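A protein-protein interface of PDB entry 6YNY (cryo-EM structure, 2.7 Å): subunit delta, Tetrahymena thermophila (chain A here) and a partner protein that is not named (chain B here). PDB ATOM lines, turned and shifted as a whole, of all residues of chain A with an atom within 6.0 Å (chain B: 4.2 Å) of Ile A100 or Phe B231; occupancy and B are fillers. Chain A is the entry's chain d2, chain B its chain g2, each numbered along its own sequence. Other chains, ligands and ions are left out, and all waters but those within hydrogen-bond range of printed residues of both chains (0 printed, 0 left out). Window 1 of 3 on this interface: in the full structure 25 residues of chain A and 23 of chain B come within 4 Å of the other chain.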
ATOM      1  N   SER A  68     -32.986  10.076 -14.249  1.00  0.00           N
ATOM      2  CA  SER A  68     -33.389   9.910 -12.861  1.00  0.00           C
ATOM      3  C   SER A  68     -32.703   8.688 -12.272  1.00  0.00           C
ATOM      4  O   SER A  68     -32.342   7.755 -12.994  1.00  0.00           O
ATOM      5  CB  SER A  68     -34.910   9.773 -12.742  1.00  0.00           C
ATOM      6  OG  SER A  68     -35.406   8.845 -13.690  1.00  0.00           O
ATOM      7  N   LEU A  69     -32.533   8.708 -10.952  1.00  0.00           N
ATOM      8  CA  LEU A  69     -31.989   7.590 -10.199  1.00  0.00           C
ATOM      9  C   LEU A  69     -33.088   6.936  -9.376  1.00  0.00           C
ATOM     10  O   LEU A  69     -34.047   7.589  -8.957  1.00  0.00           O
ATOM     11  CB  LEU A  69     -30.863   8.033  -9.262  1.00  0.00           C
ATOM     12  CG  LEU A  69     -29.681   8.779  -9.874  1.00  0.00           C
ATOM     13  CD1 LEU A  69     -29.942  10.268  -9.893  1.00  0.00           C
ATOM     14  CD2 LEU A  69     -28.418   8.472  -9.098  1.00  0.00           C
ATOM     15  N   TYR A  70     -32.940   5.633  -9.149  1.00  0.00           N
ATOM     16  CA  TYR A  70     -33.887   4.891  -8.335  1.00  0.00           C
ATOM     17  C   TYR A  70     -33.143   3.799  -7.585  1.00  0.00           C
ATOM     18  O   TYR A  70     -32.050   3.380  -7.974  1.00  0.00           O
ATOM     19  CB  TYR A  70     -35.013   4.290  -9.180  1.00  0.00           C
ATOM     20  CG  TYR A  70     -35.751   5.305 -10.019  1.00  0.00           C
ATOM     21  CD1 TYR A  70     -36.864   5.964  -9.524  1.00  0.00           C
ATOM     22  CD2 TYR A  70     -35.329   5.606 -11.305  1.00  0.00           C
ATOM     23  CE1 TYR A  70     -37.540   6.894 -10.287  1.00  0.00           C
ATOM     24  CE2 TYR A  70     -35.997   6.533 -12.074  1.00  0.00           C
ATOM     25  CZ  TYR A  70     -37.101   7.174 -11.561  1.00  0.00           C
ATOM     26  OH  TYR A  70     -37.771   8.100 -12.327  1.00  0.00           O
ATOM     27  N   VAL A  71     -33.753   3.347  -6.493  1.00  0.00           N
ATOM     28  CA  VAL A  71     -33.234   2.252  -5.683  1.00  0.00           C
ATOM     29  C   VAL A  71     -34.407   1.337  -5.368  1.00  0.00           C
ATOM     30  O   VAL A  71     -35.328   1.731  -4.644  1.00  0.00           O
ATOM     31  CB  VAL A  71     -32.565   2.743  -4.393  1.00  0.00           C
ATOM     32  CG1 VAL A  71     -32.220   1.575  -3.494  1.00  0.00           C
ATOM     33  CG2 VAL A  71     -31.321   3.543  -4.728  1.00  0.00           C
ATOM     34  N   TRP A  98     -29.960  -1.380  -7.888  1.00  0.00           N
ATOM     35  CA  TRP A  98     -29.853   0.031  -8.219  1.00  0.00           C
ATOM     36  C   TRP A  98     -30.279   0.245  -9.664  1.00  0.00           C
ATOM     37  O   TRP A  98     -30.050  -0.606 -10.528  1.00  0.00           O
ATOM     38  CB  TRP A  98     -28.422   0.535  -8.022  1.00  0.00           C
ATOM     39  CG  TRP A  98     -27.913   0.402  -6.621  1.00  0.00           C
ATOM     40  CD1 TRP A  98     -27.760   1.403  -5.709  1.00  0.00           C
ATOM     41  CD2 TRP A  98     -27.488  -0.801  -5.969  1.00  0.00           C
ATOM     42  NE1 TRP A  98     -27.265   0.901  -4.531  1.00  0.00           N
ATOM     43  CE2 TRP A  98     -27.091  -0.451  -4.665  1.00  0.00           C
ATOM     44  CE3 TRP A  98     -27.406  -2.139  -6.363  1.00  0.00           C
ATOM     45  CZ2 TRP A  98     -26.619  -1.389  -3.752  1.00  0.00           C
ATOM     46  CZ3 TRP A  98     -26.937  -3.069  -5.454  1.00  0.00           C
ATOM     47  CH2 TRP A  98     -26.550  -2.690  -4.165  1.00  0.00           C
ATOM     48  N   VAL A  99     -30.900   1.392  -9.922  1.00  0.00           N
ATOM     49  CA  VAL A  99     -31.371   1.751 -11.252  1.00  0.00           C
ATOM     50  C   VAL A  99     -30.930   3.172 -11.558  1.00  0.00           C
ATOM     51  O   VAL A  99     -31.061   4.064 -10.714  1.00  0.00           O
ATOM     52  CB  VAL A  99     -32.900   1.630 -11.371  1.00  0.00           C
ATOM     53  CG1 VAL A  99     -33.344   1.972 -12.781  1.00  0.00           C
ATOM     54  CG2 VAL A  99     -33.354   0.240 -10.984  1.00  0.00           C
ATOM     55  N   ILE A 100     -30.412   3.380 -12.764  1.00  0.00           N
ATOM     56  CA  ILE A 100     -29.963   4.689 -13.218  1.00  0.00           C
ATOM     57  C   ILE A 100     -30.415   4.865 -14.657  1.00  0.00           C
ATOM     58  O   ILE A 100     -30.249   3.958 -15.480  1.00  0.00           O
ATOM     59  CB  ILE A 100     -28.436   4.856 -13.106  1.00  0.00           C
ATOM     60  CG1 ILE A 100     -27.970   4.509 -11.692  1.00  0.00           C
ATOM     61  CG2 ILE A 100     -28.030   6.281 -13.458  1.00  0.00           C
ATOM     62  CD1 ILE A 100     -26.481   4.645 -11.495  1.00  0.00           C
ATOM     63  N   VAL A 101     -30.986   6.023 -14.960  1.00  0.00           N
ATOM     64  CA  VAL A 101     -31.424   6.365 -16.306  1.00  0.00           C
ATOM     65  C   VAL A 101     -30.477   7.448 -16.804  1.00  0.00           C
ATOM     66  O   VAL A 101     -30.633   8.630 -16.477  1.00  0.00           O
ATOM     67  CB  VAL A 101     -32.884   6.826 -16.336  1.00  0.00           C
ATOM     68  CG1 VAL A 101     -33.250   7.327 -17.722  1.00  0.00           C
ATOM     69  CG2 VAL A 101     -33.800   5.688 -15.920  1.00  0.00           C
ATOM     70  N   HIS A 102     -29.494   7.043 -17.601  1.00  0.00           N
ATOM     71  CA  HIS A 102     -28.465   7.960 -18.057  1.00  0.00           C
ATOM     72  C   HIS A 102     -29.080   9.067 -18.911  1.00  0.00           C
ATOM     73  O   HIS A 102     -30.251   9.024 -19.295  1.00  0.00           O
ATOM     74  CB  HIS A 102     -27.400   7.202 -18.847  1.00  0.00           C
ATOM     75  CG  HIS A 102     -26.707   6.141 -18.051  1.00  0.00           C
ATOM     76  ND1 HIS A 102     -25.577   6.390 -17.302  1.00  0.00           N
ATOM     77  CD2 HIS A 102     -26.988   4.827 -17.883  1.00  0.00           C
ATOM     78  CE1 HIS A 102     -25.192   5.274 -16.709  1.00  0.00           C
ATOM     79  NE2 HIS A 102     -26.030   4.310 -17.046  1.00  0.00           N
ATOM     80  N   THR A 106     -30.908   5.865 -21.641  1.00  0.00           N
ATOM     81  CA  THR A 106     -30.455   4.513 -21.342  1.00  0.00           C
ATOM     82  C   THR A 106     -30.685   4.213 -19.871  1.00  0.00           C
ATOM     83  O   THR A 106     -30.299   5.004 -19.006  1.00  0.00           O
ATOM     84  CB  THR A 106     -28.971   4.336 -21.687  1.00  0.00           C
ATOM     85  OG1 THR A 106     -28.790   4.436 -23.105  1.00  0.00           O
ATOM     86  CG2 THR A 106     -28.468   2.983 -21.205  1.00  0.00           C
ATOM     87  N   CYS A 107     -31.308   3.070 -19.594  1.00  0.00           N
ATOM     88  CA  CYS A 107     -31.590   2.627 -18.237  1.00  0.00           C
ATOM     89  C   CYS A 107     -30.891   1.300 -17.977  1.00  0.00           C
ATOM     90  O   CYS A 107     -30.922   0.398 -18.819  1.00  0.00           O
ATOM     91  CB  CYS A 107     -33.095   2.471 -18.008  1.00  0.00           C
ATOM     92  SG  CYS A 107     -33.860   1.151 -18.978  1.00  0.00           S
ATOM     93  N   GLU A 108     -30.264   1.188 -16.809  1.00  0.00           N
ATOM     94  CA  GLU A 108     -29.545  -0.016 -16.414  1.00  0.00           C
ATOM     95  C   GLU A 108     -30.064  -0.498 -15.070  1.00  0.00           C
ATOM     96  O   GLU A 108     -30.165   0.286 -14.122  1.00  0.00           O
ATOM     97  CB  GLU A 108     -28.039   0.244 -16.337  1.00  0.00           C
ATOM     98  CG  GLU A 108     -27.661   1.455 -15.514  1.00  0.00           C
ATOM     99  CD  GLU A 108     -26.164   1.640 -15.406  1.00  0.00           C
ATOM    100  OE1 GLU A 108     -25.427   0.643 -15.557  1.00  0.00           O
ATOM    101  OE2 GLU A 108     -25.722   2.784 -15.178  1.00  0.00           O
ATOM    102  N   ILE A 109     -30.391  -1.785 -14.995  1.00  0.00           N
ATOM    103  CA  ILE A 109     -30.895  -2.410 -13.778  1.00  0.00           C
ATOM    104  C   ILE A 109     -29.829  -3.371 -13.272  1.00  0.00           C
ATOM    105  O   ILE A 109     -29.469  -4.330 -13.965  1.00  0.00           O
ATOM    106  CB  ILE A 109     -32.223  -3.143 -14.020  1.00  0.00           C
ATOM    107  CG1 ILE A 109     -33.344  -2.152 -14.346  1.00  0.00           C
ATOM    108  CG2 ILE A 109     -32.597  -3.980 -12.804  1.00  0.00           C
ATOM    109  CD1 ILE A 109     -33.252  -1.539 -15.728  1.00  0.00           C
ATOM    110  N   VAL B  72     -21.817   4.741 -12.247  1.00  0.00           N
ATOM    111  CA  VAL B  72     -21.778   5.972 -11.466  1.00  0.00           C
ATOM    112  C   VAL B  72     -20.847   6.980 -12.120  1.00  0.00           C
ATOM    113  O   VAL B  72     -21.128   8.183 -12.151  1.00  0.00           O
ATOM    114  CB  VAL B  72     -21.354   5.670 -10.017  1.00  0.00           C
ATOM    115  CG1 VAL B  72     -21.307   6.949  -9.201  1.00  0.00           C
ATOM    116  CG2 VAL B  72     -22.300   4.665  -9.388  1.00  0.00           C
ATOM    117  N   MET B  75     -22.810   8.513 -15.367  1.00  0.00           N
ATOM    118  CA  MET B  75     -23.861   9.480 -15.065  1.00  0.00           C
ATOM    119  C   MET B  75     -23.277  10.756 -14.472  1.00  0.00           C
ATOM    120  O   MET B  75     -23.722  11.861 -14.799  1.00  0.00           O
ATOM    121  CB  MET B  75     -24.890   8.862 -14.118  1.00  0.00           C
ATOM    122  CG  MET B  75     -24.346   8.461 -12.756  1.00  0.00           C
ATOM    123  SD  MET B  75     -24.222   9.828 -11.583  1.00  0.00           S
ATOM    124  CE  MET B  75     -25.939  10.304 -11.414  1.00  0.00           C
ATOM    125  N   SER B 227     -30.015   8.451  -1.231  1.00  0.00           N
ATOM    126  CA  SER B 227     -29.468   7.946  -2.484  1.00  0.00           C
ATOM    127  C   SER B 227     -27.969   8.190  -2.575  1.00  0.00           C
ATOM    128  O   SER B 227     -27.229   7.355  -3.106  1.00  0.00           O
ATOM    129  CB  SER B 227     -30.187   8.597  -3.662  1.00  0.00           C
ATOM    130  OG  SER B 227     -29.715   8.083  -4.894  1.00  0.00           O
ATOM    131  N   LYS B 228     -27.503   9.331  -2.064  1.00  0.00           N
ATOM    132  CA  LYS B 228     -26.083   9.653  -2.158  1.00  0.00           C
ATOM    133  C   LYS B 228     -25.236   8.607  -1.445  1.00  0.00           C
ATOM    134  O   LYS B 228     -24.183   8.203  -1.950  1.00  0.00           O
ATOM    135  CB  LYS B 228     -25.829  11.043  -1.577  1.00  0.00           C
ATOM    136  CG  LYS B 228     -26.136  11.159  -0.095  1.00  0.00           C
ATOM    137  CD  LYS B 228     -26.322  12.607   0.329  1.00  0.00           C
ATOM    138  CE  LYS B 228     -25.068  13.431   0.116  1.00  0.00           C
ATOM    139  NZ  LYS B 228     -25.267  14.848   0.522  1.00  0.00           N
ATOM    140  N   ASN B 229     -25.679   8.157  -0.272  1.00  0.00           N
ATOM    141  CA  ASN B 229     -24.912   7.172   0.477  1.00  0.00           C
ATOM    142  C   ASN B 229     -25.062   5.775  -0.107  1.00  0.00           C
ATOM    143  O   ASN B 229     -24.121   4.976  -0.044  1.00  0.00           O
ATOM    144  CB  ASN B 229     -25.343   7.177   1.943  1.00  0.00           C
ATOM    145  CG  ASN B 229     -25.171   8.535   2.593  1.00  0.00           C
ATOM    146  OD1 ASN B 229     -26.119   9.313   2.691  1.00  0.00           O
ATOM    147  ND2 ASN B 229     -23.955   8.828   3.036  1.00  0.00           N
ATOM    148  N   TYR B 230     -26.226   5.464  -0.677  1.00  0.00           N
ATOM    149  CA  TYR B 230     -26.447   4.138  -1.242  1.00  0.00           C
ATOM    150  C   TYR B 230     -25.602   3.932  -2.493  1.00  0.00           C
ATOM    151  O   TYR B 230     -24.824   2.976  -2.584  1.00  0.00           O
ATOM    152  CB  TYR B 230     -27.930   3.942  -1.556  1.00  0.00           C
ATOM    153  CG  TYR B 230     -28.828   3.836  -0.341  1.00  0.00           C
ATOM    154  CD1 TYR B 230     -28.307   3.848   0.945  1.00  0.00           C
ATOM    155  CD2 TYR B 230     -30.201   3.711  -0.485  1.00  0.00           C
ATOM    156  CE1 TYR B 230     -29.127   3.746   2.049  1.00  0.00           C
ATOM    157  CE2 TYR B 230     -31.029   3.608   0.613  1.00  0.00           C
ATOM    158  CZ  TYR B 230     -30.488   3.625   1.877  1.00  0.00           C
ATOM    159  OH  TYR B 230     -31.314   3.522   2.970  1.00  0.00           O
ATOM    160  N   PHE B 231     -25.742   4.828  -3.473  1.00  0.00           N
ATOM    161  CA  PHE B 231     -24.974   4.697  -4.705  1.00  0.00           C
ATOM    162  C   PHE B 231     -23.476   4.787  -4.459  1.00  0.00           C
ATOM    163  O   PHE B 231     -22.692   4.350  -5.308  1.00  0.00           O
ATOM    164  CB  PHE B 231     -25.409   5.764  -5.708  1.00  0.00           C
ATOM    165  CG  PHE B 231     -26.664   5.412  -6.451  1.00  0.00           C
ATOM    166  CD1 PHE B 231     -27.882   5.945  -6.073  1.00  0.00           C
ATOM    167  CD2 PHE B 231     -26.624   4.538  -7.523  1.00  0.00           C
ATOM    168  CE1 PHE B 231     -29.036   5.617  -6.754  1.00  0.00           C
ATOM    169  CE2 PHE B 231     -27.777   4.208  -8.207  1.00  0.00           C
ATOM    170  CZ  PHE B 231     -28.984   4.748  -7.821  1.00  0.00           C
ATOM    171  N   PHE B 232     -23.057   5.339  -3.319  1.00  0.00           N
ATOM    172  CA  PHE B 232     -21.640   5.320  -2.976  1.00  0.00           C
ATOM    173  C   PHE B 232     -21.155   3.891  -2.779  1.00  0.00           C
ATOM    174  O   PHE B 232     -20.082   3.516  -3.266  1.00  0.00           O
ATOM    175  CB  PHE B 232     -21.391   6.153  -1.721  1.00  0.00           C
ATOM    176  CG  PHE B 232     -20.017   5.982  -1.146  1.00  0.00           C
ATOM    177  CD1 PHE B 232     -19.827   5.278   0.029  1.00  0.00           C
ATOM    178  CD2 PHE B 232     -18.914   6.514  -1.788  1.00  0.00           C
ATOM    179  CE1 PHE B 232     -18.564   5.117   0.557  1.00  0.00           C
ATOM    180  CE2 PHE B 232     -17.649   6.355  -1.265  1.00  0.00           C
ATOM    181  CZ  PHE B 232     -17.472   5.656  -0.091  1.00  0.00           C
ATOM    182  N   GLU B 233     -21.936   3.077  -2.066  1.00  0.00           N
ATOM    183  CA  GLU B 233     -21.599   1.667  -1.910  1.00  0.00           C
ATOM    184  C   GLU B 233     -21.471   0.988  -3.266  1.00  0.00           C
ATOM    185  O   GLU B 233     -20.479   0.306  -3.545  1.00  0.00           O
ATOM    186  CB  GLU B 233     -22.661   0.970  -1.062  1.00  0.00           C
ATOM    187  CG  GLU B 233     -22.770   1.498   0.353  1.00  0.00           C
ATOM    188  CD  GLU B 233     -23.923   0.875   1.115  1.00  0.00           C
ATOM    189  OE1 GLU B 233     -24.977   1.534   1.242  1.00  0.00           O
ATOM    190  OE2 GLU B 233     -23.779  -0.275   1.576  1.00  0.00           O
ATOM    191  N   LEU B 234     -22.478   1.165  -4.124  1.00  0.00           N
ATOM    192  CA  LEU B 234     -22.424   0.602  -5.468  1.00  0.00           C
ATOM    193  C   LEU B 234     -21.160   1.039  -6.195  1.00  0.00           C
ATOM    194  O   LEU B 234     -20.514   0.238  -6.879  1.00  0.00           O
ATOM    195  CB  LEU B 234     -23.662   1.028  -6.256  1.00  0.00           C
ATOM    196  CG  LEU B 234     -23.783   0.490  -7.681  1.00  0.00           C
ATOM    197  CD1 LEU B 234     -24.080  -0.996  -7.652  1.00  0.00           C
ATOM    198  CD2 LEU B 234     -24.849   1.243  -8.453  1.00  0.00           C
ATOM    199  N   TYR B 235     -20.791   2.314  -6.056  1.00  0.00           N
ATOM    200  CA  TYR B 235     -19.590   2.815  -6.714  1.00  0.00           C
ATOM    201  C   TYR B 235     -18.336   2.150  -6.161  1.00  0.00           C
ATOM    202  O   TYR B 235     -17.393   1.872  -6.911  1.00  0.00           O
ATOM    203  CB  TYR B 235     -19.510   4.331  -6.551  1.00  0.00           C
ATOM    204  CG  TYR B 235     -18.168   4.921  -6.907  1.00  0.00           C
ATOM    205  CD1 TYR B 235     -17.842   5.210  -8.224  1.00  0.00           C
ATOM    206  CD2 TYR B 235     -17.228   5.198  -5.923  1.00  0.00           C
ATOM    207  CE1 TYR B 235     -16.617   5.754  -8.554  1.00  0.00           C
ATOM    208  CE2 TYR B 235     -16.001   5.740  -6.243  1.00  0.00           C
ATOM    209  CZ  TYR B 235     -15.700   6.017  -7.559  1.00  0.00           C
ATOM    210  OH  TYR B 235     -14.478   6.559  -7.884  1.00  0.00           O
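Of the 11 printed residues of chain B, 4 touch a printed residue of chain A.
Printed residues of chain B that touch a printed residue of chain A: Met B75, Tyr B230, Phe B231 and Leu B234.
Of the printed residues of chain B, Tyr A70 touches Phe B231 (3.4 Å).
Of the printed residues of chain B, Trp A98 touches Tyr B230 (3.7 Å), Phe B231 (3.7 Å) and Leu B234 (3.7 Å).
Of the printed residues of chain A, Tyr B230 touches Trp A98.
Phe B231 touches just these residues of chain A: Leu A69, Tyr A70, Val A71, Trp A98, Val A99 and Ile A100.
The nearest printed residue of chain B that does not touch Tyr A70 is Ser B227 (5.9 Å).
Met B75 touches Leu A69 (CE to CD2, 3.9 Å).
Leu A69 touches Phe B231 (CD2 to CE1, 3.7 Å).
Phe B231 touches Tyr A70 (CZ to O, 3.4 Å).
Val A71 touches Phe B231 (CG2 to CE1, 3.7 Å).
Tyr B230 touches Trp A98 (O to NE1, 3.7 Å).
Trp A98 touches Phe B231 (CB to CE2, 3.7 Å).
CD2 of Leu B234 touches CG of Trp A98, 3.7 Å away.
Val A99 touches Phe B231.
Ile A100 touches Phe B231.
His A102 touches Met B75.
The side-chain hydroxyl (OG) of Ser A68 sits at hydrogen-bond distance from the side-chain hydroxyl (OH) of Tyr A70 (2.8 Å).
The backbone NH (N) of Tyr A70 is in hydrogen-bond range of the backbone carbonyl oxygen (O) of Val A99.
N of Glu A108 is in hydrogen-bond range of O of Ile A100 (3.1 Å).
A ring nitrogen (NE2) of His A102 sits at hydrogen-bond distance from the side-chain carboxylate (OE2) of Glu A108.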
